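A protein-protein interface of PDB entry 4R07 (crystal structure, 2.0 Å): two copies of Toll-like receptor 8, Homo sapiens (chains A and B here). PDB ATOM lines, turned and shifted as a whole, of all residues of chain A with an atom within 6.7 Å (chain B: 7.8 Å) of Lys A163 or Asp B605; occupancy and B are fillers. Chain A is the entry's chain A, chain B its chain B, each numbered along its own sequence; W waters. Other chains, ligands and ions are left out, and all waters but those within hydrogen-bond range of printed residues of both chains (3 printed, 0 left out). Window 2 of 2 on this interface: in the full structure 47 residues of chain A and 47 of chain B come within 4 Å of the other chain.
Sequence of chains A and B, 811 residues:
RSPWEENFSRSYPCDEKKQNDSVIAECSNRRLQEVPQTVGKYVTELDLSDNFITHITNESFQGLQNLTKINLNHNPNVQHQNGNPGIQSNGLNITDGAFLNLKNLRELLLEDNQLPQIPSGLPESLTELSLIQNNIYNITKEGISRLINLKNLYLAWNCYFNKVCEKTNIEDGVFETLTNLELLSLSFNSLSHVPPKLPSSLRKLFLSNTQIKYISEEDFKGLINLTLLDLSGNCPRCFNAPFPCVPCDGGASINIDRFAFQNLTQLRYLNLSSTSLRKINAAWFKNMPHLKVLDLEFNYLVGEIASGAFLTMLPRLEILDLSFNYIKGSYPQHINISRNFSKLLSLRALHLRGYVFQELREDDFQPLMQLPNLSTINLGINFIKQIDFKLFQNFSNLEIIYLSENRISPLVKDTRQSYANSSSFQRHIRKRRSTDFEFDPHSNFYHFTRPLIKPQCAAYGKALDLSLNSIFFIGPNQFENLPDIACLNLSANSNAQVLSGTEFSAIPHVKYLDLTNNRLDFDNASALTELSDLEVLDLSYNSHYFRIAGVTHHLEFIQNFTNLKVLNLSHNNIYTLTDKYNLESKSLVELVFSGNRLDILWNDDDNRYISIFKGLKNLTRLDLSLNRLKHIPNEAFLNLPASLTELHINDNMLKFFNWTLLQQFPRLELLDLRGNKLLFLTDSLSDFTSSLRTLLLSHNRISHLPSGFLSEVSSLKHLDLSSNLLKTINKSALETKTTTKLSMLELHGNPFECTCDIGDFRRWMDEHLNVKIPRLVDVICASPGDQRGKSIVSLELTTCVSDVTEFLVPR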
ATOM      1  N   GLN A 133       4.478   7.215  29.750  1.00  0.00           N
ATOM      2  CA  GLN A 133       3.386   8.189  29.791  1.00  0.00           C
ATOM      3  C   GLN A 133       3.285   8.842  31.165  1.00  0.00           C
ATOM      4  O   GLN A 133       2.224   8.881  31.759  1.00  0.00           O
ATOM      5  CB  GLN A 133       2.043   7.549  29.435  1.00  0.00           C
ATOM      6  CG  GLN A 133       1.688   7.639  27.943  1.00  0.00           C
ATOM      7  CD  GLN A 133       1.498   9.095  27.486  1.00  0.00           C
ATOM      8  OE1 GLN A 133       1.483  10.024  28.303  1.00  0.00           O
ATOM      9  NE2 GLN A 133       1.332   9.298  26.187  1.00  0.00           N
ATOM     10  N   ASN A 134       4.416   9.296  31.683  1.00  0.00           N
ATOM     11  CA  ASN A 134       4.425  10.106  32.892  1.00  0.00           C
ATOM     12  C   ASN A 134       5.068  11.460  32.607  1.00  0.00           C
ATOM     13  O   ASN A 134       5.159  11.896  31.443  1.00  0.00           O
ATOM     14  CB  ASN A 134       5.153   9.362  34.009  1.00  0.00           C
ATOM     15  CG  ASN A 134       4.302   8.279  34.641  1.00  0.00           C
ATOM     16  OD1 ASN A 134       3.289   8.578  35.288  1.00  0.00           O
ATOM     17  ND2 ASN A 134       4.692   7.007  34.452  1.00  0.00           N
ATOM     18  N   ASN A 135       5.396  12.193  33.663  1.00  0.00           N
ATOM     19  CA  ASN A 135       6.010  13.505  33.489  1.00  0.00           C
ATOM     20  C   ASN A 135       7.474  13.511  33.955  1.00  0.00           C
ATOM     21  O   ASN A 135       7.931  14.463  34.552  1.00  0.00           O
ATOM     22  CB  ASN A 135       5.210  14.575  34.241  1.00  0.00           C
ATOM     23  CG  ASN A 135       3.789  14.678  33.752  1.00  0.00           C
ATOM     24  OD1 ASN A 135       3.494  14.505  32.569  1.00  0.00           O
ATOM     25  ND2 ASN A 135       2.894  14.963  34.656  1.00  0.00           N
ATOM     26  N   ILE A 136       8.192  12.430  33.672  1.00  0.00           N
ATOM     27  CA  ILE A 136       9.561  12.238  34.173  1.00  0.00           C
ATOM     28  C   ILE A 136      10.612  12.737  33.181  1.00  0.00           C
ATOM     29  O   ILE A 136      10.718  12.222  32.071  1.00  0.00           O
ATOM     30  CB  ILE A 136       9.818  10.763  34.497  1.00  0.00           C
ATOM     31  CG1 ILE A 136       8.813  10.282  35.539  1.00  0.00           C
ATOM     32  CG2 ILE A 136      11.213  10.565  35.077  1.00  0.00           C
ATOM     33  CD1 ILE A 136       8.773   8.774  35.697  1.00  0.00           C
ATOM     34  N   TYR A 137      11.331  13.782  33.568  1.00  0.00           N
ATOM     35  CA  TYR A 137      12.279  14.421  32.686  1.00  0.00           C
ATOM     36  C   TYR A 137      13.700  14.289  33.198  1.00  0.00           C
ATOM     37  O   TYR A 137      14.613  14.826  32.615  1.00  0.00           O
ATOM     38  CB  TYR A 137      11.924  15.880  32.489  1.00  0.00           C
ATOM     39  CG  TYR A 137      10.445  16.106  32.230  1.00  0.00           C
ATOM     40  CD1 TYR A 137       9.758  15.362  31.271  1.00  0.00           C
ATOM     41  CD2 TYR A 137       9.718  17.041  32.983  1.00  0.00           C
ATOM     42  CE1 TYR A 137       8.397  15.575  31.044  1.00  0.00           C
ATOM     43  CE2 TYR A 137       8.354  17.200  32.818  1.00  0.00           C
ATOM     44  CZ  TYR A 137       7.691  16.462  31.849  1.00  0.00           C
ATOM     45  OH  TYR A 137       6.337  16.663  31.648  1.00  0.00           O
ATOM     46  N   TRP A 157       7.568   8.065  26.103  1.00  0.00           N
ATOM     47  CA  TRP A 157       6.372   8.900  26.022  1.00  0.00           C
ATOM     48  C   TRP A 157       6.203   9.723  27.284  1.00  0.00           C
ATOM     49  O   TRP A 157       5.068   9.943  27.747  1.00  0.00           O
ATOM     50  CB  TRP A 157       5.094   8.059  25.774  1.00  0.00           C
ATOM     51  CG  TRP A 157       4.955   7.466  24.434  1.00  0.00           C
ATOM     52  CD1 TRP A 157       5.257   6.193  24.079  1.00  0.00           C
ATOM     53  CD2 TRP A 157       4.369   8.075  23.274  1.00  0.00           C
ATOM     54  NE1 TRP A 157       4.952   5.985  22.762  1.00  0.00           N
ATOM     55  CE2 TRP A 157       4.394   7.125  22.250  1.00  0.00           C
ATOM     56  CE3 TRP A 157       3.779   9.320  23.023  1.00  0.00           C
ATOM     57  CZ2 TRP A 157       3.897   7.382  20.985  1.00  0.00           C
ATOM     58  CZ3 TRP A 157       3.310   9.589  21.750  1.00  0.00           C
ATOM     59  CH2 TRP A 157       3.359   8.631  20.752  1.00  0.00           C
ATOM     60  N   ASN A 158       7.314  10.256  27.784  1.00  0.00           N
ATOM     61  CA  ASN A 158       7.256  11.266  28.823  1.00  0.00           C
ATOM     62  C   ASN A 158       7.351  12.711  28.297  1.00  0.00           C
ATOM     63  O   ASN A 158       6.833  13.620  28.922  1.00  0.00           O
ATOM     64  CB  ASN A 158       8.280  10.993  29.920  1.00  0.00           C
ATOM     65  CG  ASN A 158       7.832   9.888  30.887  1.00  0.00           C
ATOM     66  OD1 ASN A 158       7.569  10.134  32.052  1.00  0.00           O
ATOM     67  ND2 ASN A 158       7.761   8.654  30.396  1.00  0.00           N
ATOM     68  N   CYS A 159       7.971  12.945  27.152  1.00  0.00           N
ATOM     69  CA  CYS A 159       8.020  14.317  26.620  1.00  0.00           C
ATOM     70  C   CYS A 159       8.017  14.347  25.119  1.00  0.00           C
ATOM     71  O   CYS A 159       8.969  13.902  24.498  1.00  0.00           O
ATOM     72  CB  CYS A 159       9.240  15.078  27.138  1.00  0.00           C
ATOM     73  SG  CYS A 159       9.334  16.759  26.520  1.00  0.00           S
ATOM     74  N   TYR A 160       6.942  14.867  24.525  1.00  0.00           N
ATOM     75  CA  TYR A 160       6.703  14.624  23.106  1.00  0.00           C
ATOM     76  C   TYR A 160       5.639  15.576  22.564  1.00  0.00           C
ATOM     77  O   TYR A 160       4.867  16.171  23.323  1.00  0.00           O
ATOM     78  CB  TYR A 160       6.274  13.155  22.893  1.00  0.00           C
ATOM     79  CG  TYR A 160       4.952  12.873  23.565  1.00  0.00           C
ATOM     80  CD1 TYR A 160       4.892  12.522  24.901  1.00  0.00           C
ATOM     81  CD2 TYR A 160       3.758  13.075  22.893  1.00  0.00           C
ATOM     82  CE1 TYR A 160       3.671  12.319  25.533  1.00  0.00           C
ATOM     83  CE2 TYR A 160       2.537  12.934  23.530  1.00  0.00           C
ATOM     84  CZ  TYR A 160       2.498  12.554  24.852  1.00  0.00           C
ATOM     85  OH  TYR A 160       1.297  12.419  25.493  1.00  0.00           O
ATOM     86  N   PHE A 161       5.616  15.680  21.244  1.00  0.00           N
ATOM     87  CA  PHE A 161       4.720  16.543  20.481  1.00  0.00           C
ATOM     88  C   PHE A 161       4.707  17.963  21.051  1.00  0.00           C
ATOM     89  O   PHE A 161       5.761  18.529  21.350  1.00  0.00           O
ATOM     90  CB  PHE A 161       3.301  15.945  20.414  1.00  0.00           C
ATOM     91  CG  PHE A 161       3.221  14.567  19.811  1.00  0.00           C
ATOM     92  CD1 PHE A 161       4.253  14.039  19.049  1.00  0.00           C
ATOM     93  CD2 PHE A 161       2.035  13.866  19.873  1.00  0.00           C
ATOM     94  CE1 PHE A 161       4.143  12.763  18.485  1.00  0.00           C
ATOM     95  CE2 PHE A 161       1.913  12.599  19.317  1.00  0.00           C
ATOM     96  CZ  PHE A 161       2.978  12.035  18.644  1.00  0.00           C
ATOM     97  N   ASN A 162       3.517  18.514  21.276  1.00  0.00           N
ATOM     98  CA  ASN A 162       3.393  19.796  21.918  1.00  0.00           C
ATOM     99  C   ASN A 162       3.019  19.631  23.385  1.00  0.00           C
ATOM    100  O   ASN A 162       2.469  20.561  23.986  1.00  0.00           O
ATOM    101  CB  ASN A 162       2.342  20.694  21.203  1.00  0.00           C
ATOM    102  CG  ASN A 162       2.639  20.926  19.719  1.00  0.00           C
ATOM    103  OD1 ASN A 162       1.731  20.974  18.883  1.00  0.00           O
ATOM    104  ND2 ASN A 162       3.900  21.114  19.390  1.00  0.00           N
ATOM    105  N   LYS A 163       3.379  18.511  24.008  1.00  0.00           N
ATOM    106  CA  LYS A 163       3.258  18.454  25.459  1.00  0.00           C
ATOM    107  C   LYS A 163       4.163  19.558  26.052  1.00  0.00           C
ATOM    108  O   LYS A 163       5.214  19.853  25.499  1.00  0.00           O
ATOM    109  CB  LYS A 163       3.702  17.097  26.002  1.00  0.00           C
ATOM    110  CG  LYS A 163       3.438  16.912  27.490  1.00  0.00           C
ATOM    111  CD  LYS A 163       4.015  15.604  27.998  1.00  0.00           C
ATOM    112  CE  LYS A 163       3.734  15.370  29.473  1.00  0.00           C
ATOM    113  NZ  LYS A 163       4.278  14.052  29.913  1.00  0.00           N
ATOM    114  N   VAL A 164       3.745  20.155  27.157  1.00  0.00           N
ATOM    115  CA  VAL A 164       4.614  21.042  27.900  1.00  0.00           C
ATOM    116  C   VAL A 164       5.511  20.223  28.816  1.00  0.00           C
ATOM    117  O   VAL A 164       5.061  19.657  29.789  1.00  0.00           O
ATOM    118  CB  VAL A 164       3.824  22.059  28.758  1.00  0.00           C
ATOM    119  CG1 VAL A 164       4.804  22.917  29.572  1.00  0.00           C
ATOM    120  CG2 VAL A 164       2.919  22.924  27.879  1.00  0.00           C
ATOM    121  N   CYS A 165       6.790  20.163  28.512  1.00  0.00           N
ATOM    122  CA  CYS A 165       7.665  19.266  29.256  1.00  0.00           C
ATOM    123  C   CYS A 165       9.068  19.719  29.047  1.00  0.00           C
ATOM    124  O   CYS A 165       9.297  20.613  28.292  1.00  0.00           O
ATOM    125  CB  CYS A 165       7.503  17.826  28.763  1.00  0.00           C
ATOM    126  SG  CYS A 165       7.524  17.646  26.963  1.00  0.00           S
ATOM    127  N   GLU A 166      10.000  19.157  29.798  1.00  0.00           N
ATOM    128  CA  GLU A 166      11.418  19.496  29.669  1.00  0.00           C
ATOM    129  C   GLU A 166      12.145  18.464  28.796  1.00  0.00           C
ATOM    130  O   GLU A 166      11.768  17.277  28.770  1.00  0.00           O
ATOM    131  CB  GLU A 166      12.078  19.505  31.060  1.00  0.00           C
ATOM    132  CG  GLU A 166      11.316  20.266  32.145  1.00  0.00           C
ATOM    133  CD  GLU A 166      11.225  21.748  31.876  1.00  0.00           C
ATOM    134  OE1 GLU A 166      11.996  22.259  31.035  1.00  0.00           O
ATOM    135  OE2 GLU A 166      10.402  22.417  32.533  1.00  0.00           O
ATOM    136  N   PRO A 244       2.096  16.625  15.598  1.00  0.00           N
ATOM    137  CA  PRO A 244       2.990  17.740  15.454  1.00  0.00           C
ATOM    138  C   PRO A 244       4.433  17.269  15.249  1.00  0.00           C
ATOM    139  O   PRO A 244       4.963  16.501  16.040  1.00  0.00           O
ATOM    140  CB  PRO A 244       2.844  18.521  16.769  1.00  0.00           C
ATOM    141  CG  PRO A 244       1.828  17.849  17.548  1.00  0.00           C
ATOM    142  CD  PRO A 244       1.555  16.505  16.957  1.00  0.00           C
ATOM    143  N   ASP A 436      -6.816   9.393  26.898  1.00  0.00           N
ATOM    144  CA  ASP A 436      -6.835  10.698  26.219  1.00  0.00           C
ATOM    145  C   ASP A 436      -5.451  11.087  25.670  1.00  0.00           C
ATOM    146  O   ASP A 436      -5.146  12.273  25.503  1.00  0.00           O
ATOM    147  CB  ASP A 436      -7.400  11.801  27.140  1.00  0.00           C
ATOM    148  CG  ASP A 436      -6.485  12.126  28.322  1.00  0.00           C
ATOM    149  OD1 ASP A 436      -5.391  11.528  28.421  1.00  0.00           O
ATOM    150  OD2 ASP A 436      -6.862  12.986  29.155  1.00  0.00           O
ATOM    151  N   PHE A 437      -4.614  10.080  25.411  1.00  0.00           N
ATOM    152  CA  PHE A 437      -3.572  10.191  24.384  1.00  0.00           C
ATOM    153  C   PHE A 437      -3.912   9.361  23.141  1.00  0.00           C
ATOM    154  O   PHE A 437      -4.403   8.246  23.240  1.00  0.00           O
ATOM    155  CB  PHE A 437      -2.183   9.849  24.936  1.00  0.00           C
ATOM    156  CG  PHE A 437      -2.130   8.591  25.767  1.00  0.00           C
ATOM    157  CD1 PHE A 437      -2.104   7.338  25.158  1.00  0.00           C
ATOM    158  CD2 PHE A 437      -2.026   8.667  27.154  1.00  0.00           C
ATOM    159  CE1 PHE A 437      -2.003   6.184  25.929  1.00  0.00           C
ATOM    160  CE2 PHE A 437      -1.938   7.521  27.923  1.00  0.00           C
ATOM    161  CZ  PHE A 437      -1.902   6.283  27.307  1.00  0.00           C
ATOM    162  N   GLU A 438      -3.662   9.952  21.975  1.00  0.00           N
ATOM    163  CA  GLU A 438      -4.099   9.403  20.691  1.00  0.00           C
ATOM    164  C   GLU A 438      -3.404   8.117  20.266  1.00  0.00           C
ATOM    165  O   GLU A 438      -4.000   7.317  19.563  1.00  0.00           O
ATOM    166  CB  GLU A 438      -3.896  10.464  19.590  1.00  0.00           C
ATOM    167  CG  GLU A 438      -4.238   9.990  18.185  1.00  0.00           C
ATOM    168  CD  GLU A 438      -3.981  11.043  17.111  1.00  0.00           C
ATOM    169  OE1 GLU A 438      -3.497  12.155  17.451  1.00  0.00           O
ATOM    170  OE2 GLU A 438      -4.273  10.763  15.915  1.00  0.00           O
ATOM    171  N   ILE B 600      -9.698  14.111  18.635  1.00  0.00           N
ATOM    172  CA  ILE B 600      -8.305  13.976  18.164  1.00  0.00           C
ATOM    173  C   ILE B 600      -7.737  15.318  17.742  1.00  0.00           C
ATOM    174  O   ILE B 600      -6.633  15.669  18.121  1.00  0.00           O
ATOM    175  CB  ILE B 600      -8.178  12.990  16.971  1.00  0.00           C
ATOM    176  CG1 ILE B 600      -8.541  11.574  17.439  1.00  0.00           C
ATOM    177  CG2 ILE B 600      -6.746  12.991  16.448  1.00  0.00           C
ATOM    178  CD1 ILE B 600      -8.434  10.543  16.344  1.00  0.00           C
ATOM    179  N   LEU B 601      -8.477  16.072  16.934  1.00  0.00           N
ATOM    180  CA  LEU B 601      -7.959  17.354  16.428  1.00  0.00           C
ATOM    181  C   LEU B 601      -7.542  18.335  17.543  1.00  0.00           C
ATOM    182  O   LEU B 601      -6.566  19.075  17.425  1.00  0.00           O
ATOM    183  CB  LEU B 601      -8.999  18.012  15.551  1.00  0.00           C
ATOM    184  CG  LEU B 601      -9.307  17.336  14.218  1.00  0.00           C
ATOM    185  CD1 LEU B 601     -10.680  17.777  13.738  1.00  0.00           C
ATOM    186  CD2 LEU B 601      -8.258  17.690  13.192  1.00  0.00           C
ATOM    187  N   TRP B 602      -8.268  18.285  18.636  1.00  0.00           N
ATOM    188  CA  TRP B 602      -8.009  19.099  19.807  1.00  0.00           C
ATOM    189  C   TRP B 602      -7.393  18.340  20.970  1.00  0.00           C
ATOM    190  O   TRP B 602      -7.601  18.720  22.117  1.00  0.00           O
ATOM    191  CB  TRP B 602      -9.325  19.691  20.304  1.00  0.00           C
ATOM    192  CG  TRP B 602      -9.824  20.811  19.440  1.00  0.00           C
ATOM    193  CD1 TRP B 602      -9.097  21.562  18.582  1.00  0.00           C
ATOM    194  CD2 TRP B 602     -11.138  21.349  19.432  1.00  0.00           C
ATOM    195  NE1 TRP B 602      -9.898  22.470  17.963  1.00  0.00           N
ATOM    196  CE2 TRP B 602     -11.142  22.415  18.520  1.00  0.00           C
ATOM    197  CE3 TRP B 602     -12.330  21.008  20.086  1.00  0.00           C
ATOM    198  CZ2 TRP B 602     -12.291  23.126  18.209  1.00  0.00           C
ATOM    199  CZ3 TRP B 602     -13.467  21.750  19.804  1.00  0.00           C
ATOM    200  CH2 TRP B 602     -13.432  22.786  18.868  1.00  0.00           C
ATOM    201  N   ASN B 603      -6.712  17.235  20.689  1.00  0.00           N
ATOM    202  CA  ASN B 603      -5.954  16.505  21.702  1.00  0.00           C
ATOM    203  C   ASN B 603      -4.978  17.442  22.434  1.00  0.00           C
ATOM    204  O   ASN B 603      -4.391  18.311  21.819  1.00  0.00           O
ATOM    205  CB  ASN B 603      -5.216  15.353  21.011  1.00  0.00           C
ATOM    206  CG  ASN B 603      -4.309  14.611  21.931  1.00  0.00           C
ATOM    207  OD1 ASN B 603      -3.179  15.024  22.151  1.00  0.00           O
ATOM    208  ND2 ASN B 603      -4.769  13.467  22.434  1.00  0.00           N
ATOM    209  N   ASP B 604      -4.823  17.276  23.741  1.00  0.00           N
ATOM    210  CA  ASP B 604      -3.974  18.179  24.554  1.00  0.00           C
ATOM    211  C   ASP B 604      -2.540  18.262  24.064  1.00  0.00           C
ATOM    212  O   ASP B 604      -1.859  19.228  24.337  1.00  0.00           O
ATOM    213  CB  ASP B 604      -3.883  17.692  26.009  1.00  0.00           C
ATOM    214  CG  ASP B 604      -5.215  17.706  26.724  1.00  0.00           C
ATOM    215  OD1 ASP B 604      -6.034  18.595  26.437  1.00  0.00           O
ATOM    216  OD2 ASP B 604      -5.430  16.810  27.564  1.00  0.00           O
ATOM    217  N   ASP B 605      -2.057  17.202  23.439  1.00  0.00           N
ATOM    218  CA  ASP B 605      -0.686  17.144  22.992  1.00  0.00           C
ATOM    219  C   ASP B 605      -0.438  17.795  21.620  1.00  0.00           C
ATOM    220  O   ASP B 605       0.663  17.736  21.116  1.00  0.00           O
ATOM    221  CB  ASP B 605      -0.208  15.704  22.960  1.00  0.00           C
ATOM    222  CG  ASP B 605      -0.144  15.069  24.333  1.00  0.00           C
ATOM    223  OD1 ASP B 605       0.121  15.780  25.332  1.00  0.00           O
ATOM    224  OD2 ASP B 605      -0.341  13.832  24.416  1.00  0.00           O
ATOM    225  N   ASP B 606      -1.445  18.410  21.008  1.00  0.00           N
ATOM    226  CA  ASP B 606      -1.303  18.940  19.641  1.00  0.00           C
ATOM    227  C   ASP B 606      -1.967  20.311  19.553  1.00  0.00           C
ATOM    228  O   ASP B 606      -3.148  20.453  19.855  1.00  0.00           O
ATOM    229  CB  ASP B 606      -1.966  17.959  18.675  1.00  0.00           C
ATOM    230  CG  ASP B 606      -1.873  18.369  17.182  1.00  0.00           C
ATOM    231  OD1 ASP B 606      -1.201  19.341  16.766  1.00  0.00           O
ATOM    232  OD2 ASP B 606      -2.497  17.631  16.396  1.00  0.00           O
ATOM    233  N   ASN B 607      -1.206  21.327  19.171  1.00  0.00           N
ATOM    234  CA  ASN B 607      -1.749  22.691  19.055  1.00  0.00           C
ATOM    235  C   ASN B 607      -2.243  23.049  17.667  1.00  0.00           C
ATOM    236  O   ASN B 607      -2.764  24.142  17.470  1.00  0.00           O
ATOM    237  CB  ASN B 607      -0.664  23.738  19.415  1.00  0.00           C
ATOM    238  CG  ASN B 607      -0.150  23.576  20.819  1.00  0.00           C
ATOM    239  OD1 ASN B 607      -0.879  23.132  21.712  1.00  0.00           O
ATOM    240  ND2 ASN B 607       1.123  23.909  21.027  1.00  0.00           N
ATOM    241  N   ARG B 608      -2.018  22.198  16.683  1.00  0.00           N
ATOM    242  CA  ARG B 608      -2.179  22.638  15.296  1.00  0.00           C
ATOM    243  C   ARG B 608      -3.600  23.062  14.918  1.00  0.00           C
ATOM    244  O   ARG B 608      -3.764  23.921  14.049  1.00  0.00           O
ATOM    245  CB  ARG B 608      -1.641  21.608  14.318  1.00  0.00           C
ATOM    246  CG  ARG B 608      -0.124  21.438  14.384  1.00  0.00           C
ATOM    247  CD  ARG B 608       0.332  20.207  13.594  1.00  0.00           C
ATOM    248  NE  ARG B 608      -0.343  19.001  14.080  1.00  0.00           N
ATOM    249  CZ  ARG B 608      -0.519  17.912  13.357  1.00  0.00           C
ATOM    250  NH1 ARG B 608      -0.064  17.861  12.117  1.00  0.00           N
ATOM    251  NH2 ARG B 608      -1.141  16.873  13.877  1.00  0.00           N
ATOM    252  N   PRO B 633     -10.356  22.160  24.932  1.00  0.00           N
ATOM    253  CA  PRO B 633      -9.378  23.053  25.545  1.00  0.00           C
ATOM    254  C   PRO B 633      -9.896  24.475  25.555  1.00  0.00           C
ATOM    255  O   PRO B 633     -10.517  24.915  24.566  1.00  0.00           O
ATOM    256  CB  PRO B 633      -8.181  22.948  24.601  1.00  0.00           C
ATOM    257  CG  PRO B 633      -8.314  21.608  23.974  1.00  0.00           C
ATOM    258  CD  PRO B 633      -9.791  21.397  23.824  1.00  0.00           C
HETATM  259  O   HOH W   1      -6.544  15.194  25.132  1.00  0.00           O
HETATM  260  O   HOH W   2      -1.643  14.402  17.297  1.00  0.00           O
HETATM  261  O   HOH W   3       0.307  14.726  27.613  1.00  0.00           O
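Gln A133 touches none of the printed residues of chain B.
Asn A135 touches none of the printed residues of chain B.
Of the printed residues of chain B, Lys A163 touches Asp B605.
Printed residues of chain B within 4 Å of Phe A437: Asn B603 (3.996 Å).
Of the printed residues of chain B, Glu A438 touches Ile B600 (3.4 Å) and Asn B603 (3.7 Å).
Asp B605 touches just these residues of chain A: Tyr A160 (2.4 Å), Phe A161 (3.3 Å), Asn A162 (3.0 Å), Lys A163 (3.9 Å) and Pro A244 (3.8 Å).
Printed residues of chain A within 4 Å of Asp B606: Asn A162 and Pro A244.
Asp B605 touches Phe A161.
Asp B606 touches Asn A162.
CB of Lys A163 touches OD1 of Asp B605 (3.9 Å).
Pro A244 touches Asp B605 (CG to O, 3.8 Å).
Asp B606 touches Pro A244 (OD1 to CG, 3.5 Å).
Arg B608 touches Pro A244.
CA of Phe A437 touches ND2 of Asn B603 (3.996 Å).
OE2 of Glu A438 touches CG2 of Ile B600, at 3.4 Å.
Glu A438 touches Asn B603.
The side-chain hydroxyl (OH) of Tyr A160 sits at hydrogen-bond distance from the side-chain carboxylate (OD2) of Asp B605 (2.4 Å).
N of Asn A162 sits at hydrogen-bond distance from O of Asp B605 (3.0 Å).
The backbone NH of Asn B607 sits at hydrogen-bond distance from the side-chain amide oxygen of Asn A162 (3.0 Å).
The backbone carbonyl oxygen (O) of Asp A436 lies within hydrogen-bond range of the side-chain amide nitrogen (ND2) of Asn B603 (3.3 Å).
Water W3 bridges OD1 of Asp B605 and OH of Tyr A160.
Water W2 lies within hydrogen-bond range of the side-chain carboxylate of Glu A438 and the side-chain carboxylate of Asp B606.
Water W1 lies within hydrogen-bond range of the backbone NH of Asp B604 (3.0 Å) and the backbone carbonyl oxygen of Asp A436 (3.3 Å).
No position is printed for both chains.
O of Asn A134 is in hydrogen-bond range of NZ of Lys A163.
The side-chain amide oxygen of Asn A135 is in hydrogen-bond range of the side-chain amino group of Lys A163, at 2.8 Å.
The side-chain amino group of Lys A163 sits at hydrogen-bond distance from the backbone carbonyl oxygen of Asn A158 (2.8 Å).
The backbone NH (N) of Tyr A160 lies within hydrogen-bond range of the side-chain sulfur (SG) of Cys A165 (3.7 Å).
The side-chain amide oxygen (OD1) of Asn B603 sits at hydrogen-bond distance from the backbone NH (N) of Asp B605 (2.8 Å).
The side-chain sulfur of Cys A165 forms a disulfide with the side-chain sulfur of Cys A159, at 2.1 Å.
Of the 19 printed residues of chain A, 8 touch a printed residue of chain B.
Hydrophobic or aromatic side chains of chain A within 4 Å of the printed part of chain B: Tyr A160, Phe A161 and Pro A244.
Of the 10 printed residues of chain B, 6 touch a printed residue of chain A.
Hydrophobic or aromatic side chains of chain B within 4 Å of the printed part of chain A: Ile B600.
Among the printed residues, 13 pairs touch across the chains.
Among the printed residues, no Asp or Glu carboxylate lies within 4 Å of a Lys or Arg side-chain nitrogen of the other chain.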
